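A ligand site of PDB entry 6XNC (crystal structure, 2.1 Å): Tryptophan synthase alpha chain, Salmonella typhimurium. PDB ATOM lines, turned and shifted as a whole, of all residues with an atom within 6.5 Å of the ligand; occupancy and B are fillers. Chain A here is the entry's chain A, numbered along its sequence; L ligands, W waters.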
ATOM      1  N   PHE A  22     -19.125  21.478  26.054  1.00  0.00           N
ATOM      2  CA  PHE A  22     -19.141  20.253  26.845  1.00  0.00           C
ATOM      3  C   PHE A  22     -18.020  19.332  26.396  1.00  0.00           C
ATOM      4  O   PHE A  22     -17.789  19.155  25.196  1.00  0.00           O
ATOM      5  CB  PHE A  22     -20.484  19.515  26.738  1.00  0.00           C
ATOM      6  CG  PHE A  22     -20.457  18.119  27.323  1.00  0.00           C
ATOM      7  CD1 PHE A  22     -20.710  17.913  28.669  1.00  0.00           C
ATOM      8  CD2 PHE A  22     -20.188  17.027  26.514  1.00  0.00           C
ATOM      9  CE1 PHE A  22     -20.681  16.634  29.211  1.00  0.00           C
ATOM     10  CE2 PHE A  22     -20.162  15.748  27.047  1.00  0.00           C
ATOM     11  CZ  PHE A  22     -20.406  15.551  28.389  1.00  0.00           C
ATOM     12  N   GLU A  49     -19.565  22.653  30.825  1.00  0.00           N
ATOM     13  CA  GLU A  49     -20.335  21.467  31.159  1.00  0.00           C
ATOM     14  C   GLU A  49     -19.406  20.266  31.032  1.00  0.00           C
ATOM     15  O   GLU A  49     -18.823  20.054  29.969  1.00  0.00           O
ATOM     16  CB  GLU A  49     -21.561  21.316  30.264  1.00  0.00           C
ATOM     17  CG  GLU A  49     -22.667  22.319  30.561  1.00  0.00           C
ATOM     18  CD  GLU A  49     -23.162  22.249  32.010  1.00  0.00           C
ATOM     19  OE1 GLU A  49     -23.167  21.141  32.583  1.00  0.00           O
ATOM     20  OE2 GLU A  49     -23.527  23.301  32.568  1.00  0.00           O
ATOM     21  N   ASP A  60     -26.637   9.715  25.163  1.00  0.00           N
ATOM     22  CA  ASP A  60     -25.581  10.250  24.312  1.00  0.00           C
ATOM     23  C   ASP A  60     -25.507   9.468  23.005  1.00  0.00           C
ATOM     24  O   ASP A  60     -25.695   8.245  22.982  1.00  0.00           O
ATOM     25  CB  ASP A  60     -24.227  10.204  25.024  1.00  0.00           C
ATOM     26  CG  ASP A  60     -24.088  11.289  26.064  1.00  0.00           C
ATOM     27  OD1 ASP A  60     -24.257  12.473  25.711  1.00  0.00           O
ATOM     28  OD2 ASP A  60     -23.823  10.965  27.245  1.00  0.00           O
ATOM     29  N   ILE A  64     -20.255  11.098  21.791  1.00  0.00           N
ATOM     30  CA  ILE A  64     -19.956  11.121  23.220  1.00  0.00           C
ATOM     31  C   ILE A  64     -19.888   9.707  23.801  1.00  0.00           C
ATOM     32  O   ILE A  64     -19.199   9.500  24.811  1.00  0.00           O
ATOM     33  CB  ILE A  64     -20.963  12.025  23.938  1.00  0.00           C
ATOM     34  CG1 ILE A  64     -20.846  13.450  23.393  1.00  0.00           C
ATOM     35  CG2 ILE A  64     -20.743  12.030  25.442  1.00  0.00           C
ATOM     36  CD1 ILE A  64     -21.739  14.457  24.081  1.00  0.00           C
ATOM     37  N   LEU A 100     -22.444  17.111  34.155  1.00  0.00           N
ATOM     38  CA  LEU A 100     -23.477  16.340  33.483  1.00  0.00           C
ATOM     39  C   LEU A 100     -23.282  14.880  33.891  1.00  0.00           C
ATOM     40  O   LEU A 100     -22.380  14.206  33.387  1.00  0.00           O
ATOM     41  CB  LEU A 100     -23.395  16.519  31.968  1.00  0.00           C
ATOM     42  CG  LEU A 100     -24.602  17.186  31.311  1.00  0.00           C
ATOM     43  CD1 LEU A 100     -24.849  18.565  31.884  1.00  0.00           C
ATOM     44  CD2 LEU A 100     -24.404  17.260  29.814  1.00  0.00           C
ATOM     45  N   LEU A 127     -26.353  18.544  36.555  1.00  0.00           N
ATOM     46  CA  LEU A 127     -27.456  17.986  35.796  1.00  0.00           C
ATOM     47  C   LEU A 127     -27.283  16.468  35.777  1.00  0.00           C
ATOM     48  O   LEU A 127     -26.214  15.971  35.411  1.00  0.00           O
ATOM     49  CB  LEU A 127     -27.487  18.546  34.368  1.00  0.00           C
ATOM     50  CG  LEU A 127     -28.728  18.366  33.492  1.00  0.00           C
ATOM     51  CD1 LEU A 127     -28.593  19.215  32.235  1.00  0.00           C
ATOM     52  CD2 LEU A 127     -28.954  16.907  33.105  1.00  0.00           C
ATOM     53  N   TYR A 175     -31.808  24.081  31.189  1.00  0.00           N
ATOM     54  CA  TYR A 175     -31.335  23.404  29.981  1.00  0.00           C
ATOM     55  C   TYR A 175     -32.499  23.320  29.003  1.00  0.00           C
ATOM     56  O   TYR A 175     -33.409  22.508  29.156  1.00  0.00           O
ATOM     57  CB  TYR A 175     -30.798  22.014  30.306  1.00  0.00           C
ATOM     58  CG  TYR A 175     -29.947  21.419  29.194  1.00  0.00           C
ATOM     59  CD1 TYR A 175     -30.524  21.017  27.997  1.00  0.00           C
ATOM     60  CD2 TYR A 175     -28.577  21.249  29.352  1.00  0.00           C
ATOM     61  CE1 TYR A 175     -29.758  20.485  26.976  1.00  0.00           C
ATOM     62  CE2 TYR A 175     -27.807  20.708  28.341  1.00  0.00           C
ATOM     63  CZ  TYR A 175     -28.400  20.336  27.159  1.00  0.00           C
ATOM     64  OH  TYR A 175     -27.639  19.794  26.152  1.00  0.00           O
ATOM     65  N   ARG A 179     -34.293  19.368  20.754  1.00  0.00           N
ATOM     66  CA  ARG A 179     -35.007  18.328  20.036  1.00  0.00           C
ATOM     67  C   ARG A 179     -35.079  17.086  20.903  1.00  0.00           C
ATOM     68  O   ARG A 179     -34.450  17.000  21.959  1.00  0.00           O
ATOM     69  CB  ARG A 179     -34.320  18.023  18.705  1.00  0.00           C
ATOM     70  CG  ARG A 179     -32.825  17.798  18.853  1.00  0.00           C
ATOM     71  CD  ARG A 179     -32.235  17.067  17.668  1.00  0.00           C
ATOM     72  NE  ARG A 179     -30.791  16.860  17.822  1.00  0.00           N
ATOM     73  CZ  ARG A 179     -30.257  15.875  18.525  1.00  0.00           C
ATOM     74  NH1 ARG A 179     -31.026  14.998  19.155  1.00  0.00           N
ATOM     75  NH2 ARG A 179     -28.937  15.768  18.611  1.00  0.00           N
ATOM     76  N   VAL A 182     -31.033  11.792  21.271  1.00  0.00           N
ATOM     77  CA  VAL A 182     -29.836  11.848  22.110  1.00  0.00           C
ATOM     78  C   VAL A 182     -28.867  12.867  21.531  1.00  0.00           C
ATOM     79  O   VAL A 182     -29.128  13.471  20.488  1.00  0.00           O
ATOM     80  CB  VAL A 182     -29.188  10.459  22.222  1.00  0.00           C
ATOM     81  CG1 VAL A 182     -30.100   9.504  22.978  1.00  0.00           C
ATOM     82  CG2 VAL A 182     -28.870   9.904  20.837  1.00  0.00           C
ATOM     83  N   THR A 183     -27.734  13.070  22.211  1.00  0.00           N
ATOM     84  CA  THR A 183     -26.771  14.069  21.786  1.00  0.00           C
ATOM     85  C   THR A 183     -26.182  13.708  20.422  1.00  0.00           C
ATOM     86  O   THR A 183     -26.060  12.527  20.063  1.00  0.00           O
ATOM     87  CB  THR A 183     -25.637  14.214  22.803  1.00  0.00           C
ATOM     88  OG1 THR A 183     -24.913  12.978  22.895  1.00  0.00           O
ATOM     89  CG2 THR A 183     -26.203  14.566  24.170  1.00  0.00           C
ATOM     90  N   GLY A 184     -25.817  14.739  19.664  1.00  0.00           N
ATOM     91  CA  GLY A 184     -25.232  14.551  18.352  1.00  0.00           C
ATOM     92  C   GLY A 184     -25.232  15.812  17.522  1.00  0.00           C
ATOM     93  O   GLY A 184     -26.274  16.458  17.351  1.00  0.00           O
ATOM     94  N   ALA A 185     -24.066  16.192  17.005  1.00  0.00           N
ATOM     95  CA  ALA A 185     -23.965  17.398  16.184  1.00  0.00           C
ATOM     96  C   ALA A 185     -24.600  17.224  14.819  1.00  0.00           C
ATOM     97  O   ALA A 185     -25.003  18.210  14.207  1.00  0.00           O
ATOM     98  CB  ALA A 185     -22.500  17.815  16.033  1.00  0.00           C
ATOM     99  N   ASN A 187     -27.441  15.989  14.099  1.00  0.00           N
ATOM    100  CA  ASN A 187     -28.884  16.171  14.171  1.00  0.00           C
ATOM    101  C   ASN A 187     -29.188  17.504  14.845  1.00  0.00           C
ATOM    102  O   ASN A 187     -28.735  17.755  15.961  1.00  0.00           O
ATOM    103  CB  ASN A 187     -29.548  15.026  14.923  1.00  0.00           C
ATOM    104  CG  ASN A 187     -30.970  14.773  14.464  1.00  0.00           C
ATOM    105  OD1 ASN A 187     -31.900  15.460  14.870  1.00  0.00           O
ATOM    106  ND2 ASN A 187     -31.137  13.769  13.611  1.00  0.00           N
ATOM    107  N   GLY A 211     -29.363  23.387  24.234  1.00  0.00           N
ATOM    108  CA  GLY A 211     -28.421  22.330  23.982  1.00  0.00           C
ATOM    109  C   GLY A 211     -29.027  21.254  23.097  1.00  0.00           C
ATOM    110  O   GLY A 211     -30.243  21.198  22.909  1.00  0.00           O
ATOM    111  N   PHE A 212     -28.139  20.387  22.572  1.00  0.00           N
ATOM    112  CA  PHE A 212     -28.409  19.321  21.612  1.00  0.00           C
ATOM    113  C   PHE A 212     -28.411  19.852  20.176  1.00  0.00           C
ATOM    114  O   PHE A 212     -29.299  20.621  19.797  1.00  0.00           O
ATOM    115  CB  PHE A 212     -29.736  18.608  21.884  1.00  0.00           C
ATOM    116  CG  PHE A 212     -29.643  17.514  22.912  1.00  0.00           C
ATOM    117  CD1 PHE A 212     -29.004  17.729  24.122  1.00  0.00           C
ATOM    118  CD2 PHE A 212     -30.204  16.270  22.667  1.00  0.00           C
ATOM    119  CE1 PHE A 212     -28.915  16.719  25.059  1.00  0.00           C
ATOM    120  CE2 PHE A 212     -30.134  15.260  23.612  1.00  0.00           C
ATOM    121  CZ  PHE A 212     -29.486  15.485  24.817  1.00  0.00           C
ATOM    122  N   GLY A 213     -27.422  19.454  19.381  1.00  0.00           N
ATOM    123  CA  GLY A 213     -27.354  19.789  17.977  1.00  0.00           C
ATOM    124  C   GLY A 213     -26.649  21.084  17.648  1.00  0.00           C
ATOM    125  O   GLY A 213     -26.401  21.350  16.460  1.00  0.00           O
ATOM    126  N   ILE A 214     -26.310  21.903  18.634  1.00  0.00           N
ATOM    127  CA  ILE A 214     -25.672  23.199  18.384  1.00  0.00           C
ATOM    128  C   ILE A 214     -24.233  22.954  17.932  1.00  0.00           C
ATOM    129  O   ILE A 214     -23.382  22.601  18.742  1.00  0.00           O
ATOM    130  CB  ILE A 214     -25.722  24.098  19.618  1.00  0.00           C
ATOM    131  CG1 ILE A 214     -27.160  24.247  20.120  1.00  0.00           C
ATOM    132  CG2 ILE A 214     -25.126  25.459  19.315  1.00  0.00           C
ATOM    133  CD1 ILE A 214     -28.115  24.812  19.107  1.00  0.00           C
ATOM    134  N   SER A 215     -23.972  23.154  16.636  1.00  0.00           N
ATOM    135  CA  SER A 215     -22.646  22.917  16.087  1.00  0.00           C
ATOM    136  C   SER A 215     -22.122  24.026  15.188  1.00  0.00           C
ATOM    137  O   SER A 215     -21.002  23.924  14.696  1.00  0.00           O
ATOM    138  CB  SER A 215     -22.628  21.594  15.307  1.00  0.00           C
ATOM    139  OG  SER A 215     -23.455  21.685  14.155  1.00  0.00           O
ATOM    140  N   ILE A 232     -25.412  25.602  24.464  1.00  0.00           N
ATOM    141  CA  ILE A 232     -24.465  24.567  24.874  1.00  0.00           C
ATOM    142  C   ILE A 232     -24.100  23.734  23.654  1.00  0.00           C
ATOM    143  O   ILE A 232     -24.975  23.374  22.857  1.00  0.00           O
ATOM    144  CB  ILE A 232     -25.057  23.679  25.996  1.00  0.00           C
ATOM    145  CG1 ILE A 232     -25.215  24.486  27.279  1.00  0.00           C
ATOM    146  CG2 ILE A 232     -24.194  22.438  26.229  1.00  0.00           C
ATOM    147  CD1 ILE A 232     -25.899  23.734  28.393  1.00  0.00           C
ATOM    148  N   SER A 233     -22.814  23.440  23.501  1.00  0.00           N
ATOM    149  CA  SER A 233     -22.317  22.638  22.378  1.00  0.00           C
ATOM    150  C   SER A 233     -21.436  21.528  22.916  1.00  0.00           C
ATOM    151  O   SER A 233     -20.427  21.795  23.584  1.00  0.00           O
ATOM    152  CB  SER A 233     -21.547  23.512  21.383  1.00  0.00           C
ATOM    153  OG  SER A 233     -21.146  22.746  20.262  1.00  0.00           O
ATOM    154  N   GLY A 234     -21.809  20.280  22.632  1.00  0.00           N
ATOM    155  CA  GLY A 234     -21.047  19.140  23.110  1.00  0.00           C
ATOM    156  C   GLY A 234     -20.416  18.307  22.025  1.00  0.00           C
ATOM    157  O   GLY A 234     -19.192  18.272  21.895  1.00  0.00           O
ATOM    158  N   SER A 235     -21.248  17.637  21.215  1.00  0.00           N
ATOM    159  CA  SER A 235     -20.724  16.714  20.210  1.00  0.00           C
ATOM    160  C   SER A 235     -19.831  17.421  19.192  1.00  0.00           C
ATOM    161  O   SER A 235     -18.868  16.831  18.712  1.00  0.00           O
ATOM    162  CB  SER A 235     -21.882  16.015  19.494  1.00  0.00           C
ATOM    163  OG  SER A 235     -22.664  15.266  20.409  1.00  0.00           O
ATOM    164  N   ALA A 236     -20.145  18.679  18.856  1.00  0.00           N
ATOM    165  CA  ALA A 236     -19.291  19.421  17.936  1.00  0.00           C
ATOM    166  C   ALA A 236     -17.896  19.620  18.516  1.00  0.00           C
ATOM    167  O   ALA A 236     -16.908  19.616  17.766  1.00  0.00           O
ATOM    168  CB  ALA A 236     -19.928  20.776  17.597  1.00  0.00           C
ATOM    169  N   VAL A 238     -16.500  17.523  20.857  1.00  0.00           N
ATOM    170  CA  VAL A 238     -15.894  16.195  21.002  1.00  0.00           C
ATOM    171  C   VAL A 238     -15.437  15.668  19.647  1.00  0.00           C
ATOM    172  O   VAL A 238     -14.446  14.924  19.567  1.00  0.00           O
ATOM    173  CB  VAL A 238     -16.873  15.243  21.697  1.00  0.00           C
ATOM    174  CG1 VAL A 238     -16.270  13.855  21.858  1.00  0.00           C
ATOM    175  CG2 VAL A 238     -17.287  15.802  23.054  1.00  0.00           C
HETATM  176  C1  LIG L   1     -24.244  18.480  26.480  1.00  0.00           C
HETATM  177  O1  LIG L   1     -23.348  17.191  24.666  1.00  0.00           O
HETATM  178  C2  LIG L   1     -24.537  17.762  25.168  1.00  0.00           C
HETATM  179  O2  LIG L   1     -25.468  18.884  27.052  1.00  0.00           O
HETATM  180  C3  LIG L   1     -25.063  18.758  24.151  1.00  0.00           C
HETATM  181  O3  LIG L   1     -25.632  18.014  23.097  1.00  0.00           O
HETATM  182  O4  LIG L   1     -25.793  17.507  20.602  1.00  0.00           O
HETATM  183  O5  LIG L   1     -24.211  19.264  21.416  1.00  0.00           O
HETATM  184  O6  LIG L   1     -23.748  16.885  21.860  1.00  0.00           O
HETATM  185  P1  LIG L   1     -24.846  17.920  21.701  1.00  0.00           P
HETATM  186  O   HOH W   1     -22.666  19.972  19.163  1.00  0.00           O
HETATM  187  O   HOH W   2     -25.823  21.239  21.420  1.00  0.00           O
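The side-chain hydroxyl (OH) of Tyr 175 is in hydrogen-bond range of an oxygen (O2) of the ligand, 2.5 Å away.
The backbone NH of Phe 212 sits close to an oxygen (O3) of the ligand (3.5 Å).
An oxygen (O4) of the ligand sits at hydrogen-bond distance from the backbone NH of Gly 184.
O5 of the ligand is in hydrogen-bond range of N of Gly 234, at 2.9 Å.
N of Gly 213 is in hydrogen-bond range of O4 of the ligand.
An oxygen (O6) of the ligand is in hydrogen-bond range of the side-chain hydroxyl (OG) of Ser 235, 2.4 Å away.
The backbone NH of Ser 235 is in hydrogen-bond range of an oxygen (O6) of the ligand, at 2.7 Å.
The backbone carbonyl oxygen of Ile 214 lies within hydrogen-bond range of the side-chain hydroxyl of Ser 233, 2.7 Å away.
The guanidinium group (NH2) of Arg 179 is in hydrogen-bond range of the backbone carbonyl oxygen (O) of Gly 184 (3.0 Å).
The side-chain hydroxyl (OG1) of Thr 183 sits at hydrogen-bond distance from the side-chain carboxylate (OD1) of Asp 60, at 2.9 Å.
O of Ser 233 lies within hydrogen-bond range of N of Phe 22.
The side-chain hydroxyl of Ser 235 lies within hydrogen-bond range of the backbone NH of Gly 184 (3.3 Å).
Phe 22 touches the ligand (CD2 to O1, 3.7 Å).
Ile 64 touches the ligand (CD1 to O1, 3.2 Å).
Leu 100 touches the ligand (CD2 to O2, 3.4 Å).
CB of Thr 183 touches O6 of the ligand, 3.4 Å away.
CG2 of Ile 232 touches O2 of the ligand, 3.9 Å away.
C of Ser 233 touches O5 of the ligand, 3.9 Å away.
Hydrophobic or aromatic side chains that line the ligand: Phe 22, Ile 64, Leu 100, Tyr 175, Phe 212 and Ile 232.
12 residues have an atom within 4 Å of the ligand: Phe 22, Ile 64, Leu 100, Tyr 175, Thr 183, Gly 184, Phe 212, Gly 213, Ile 232, Ser 233, Gly 234 and Ser 235.
The nearest printed residue that does not touch the ligand is Arg 179 (4.1 Å).
Water W1 lies within hydrogen-bond range of the backbone carbonyl oxygen (O) of Ile 214 (2.8 Å), an oxygen (O5) of the ligand (2.8 Å), the backbone NH (N) of Ala 236 (2.8 Å), the side-chain hydroxyl (OG) of Ser 233 (3.3 Å) and the backbone NH (N) of Ser 235 (3.4 Å).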
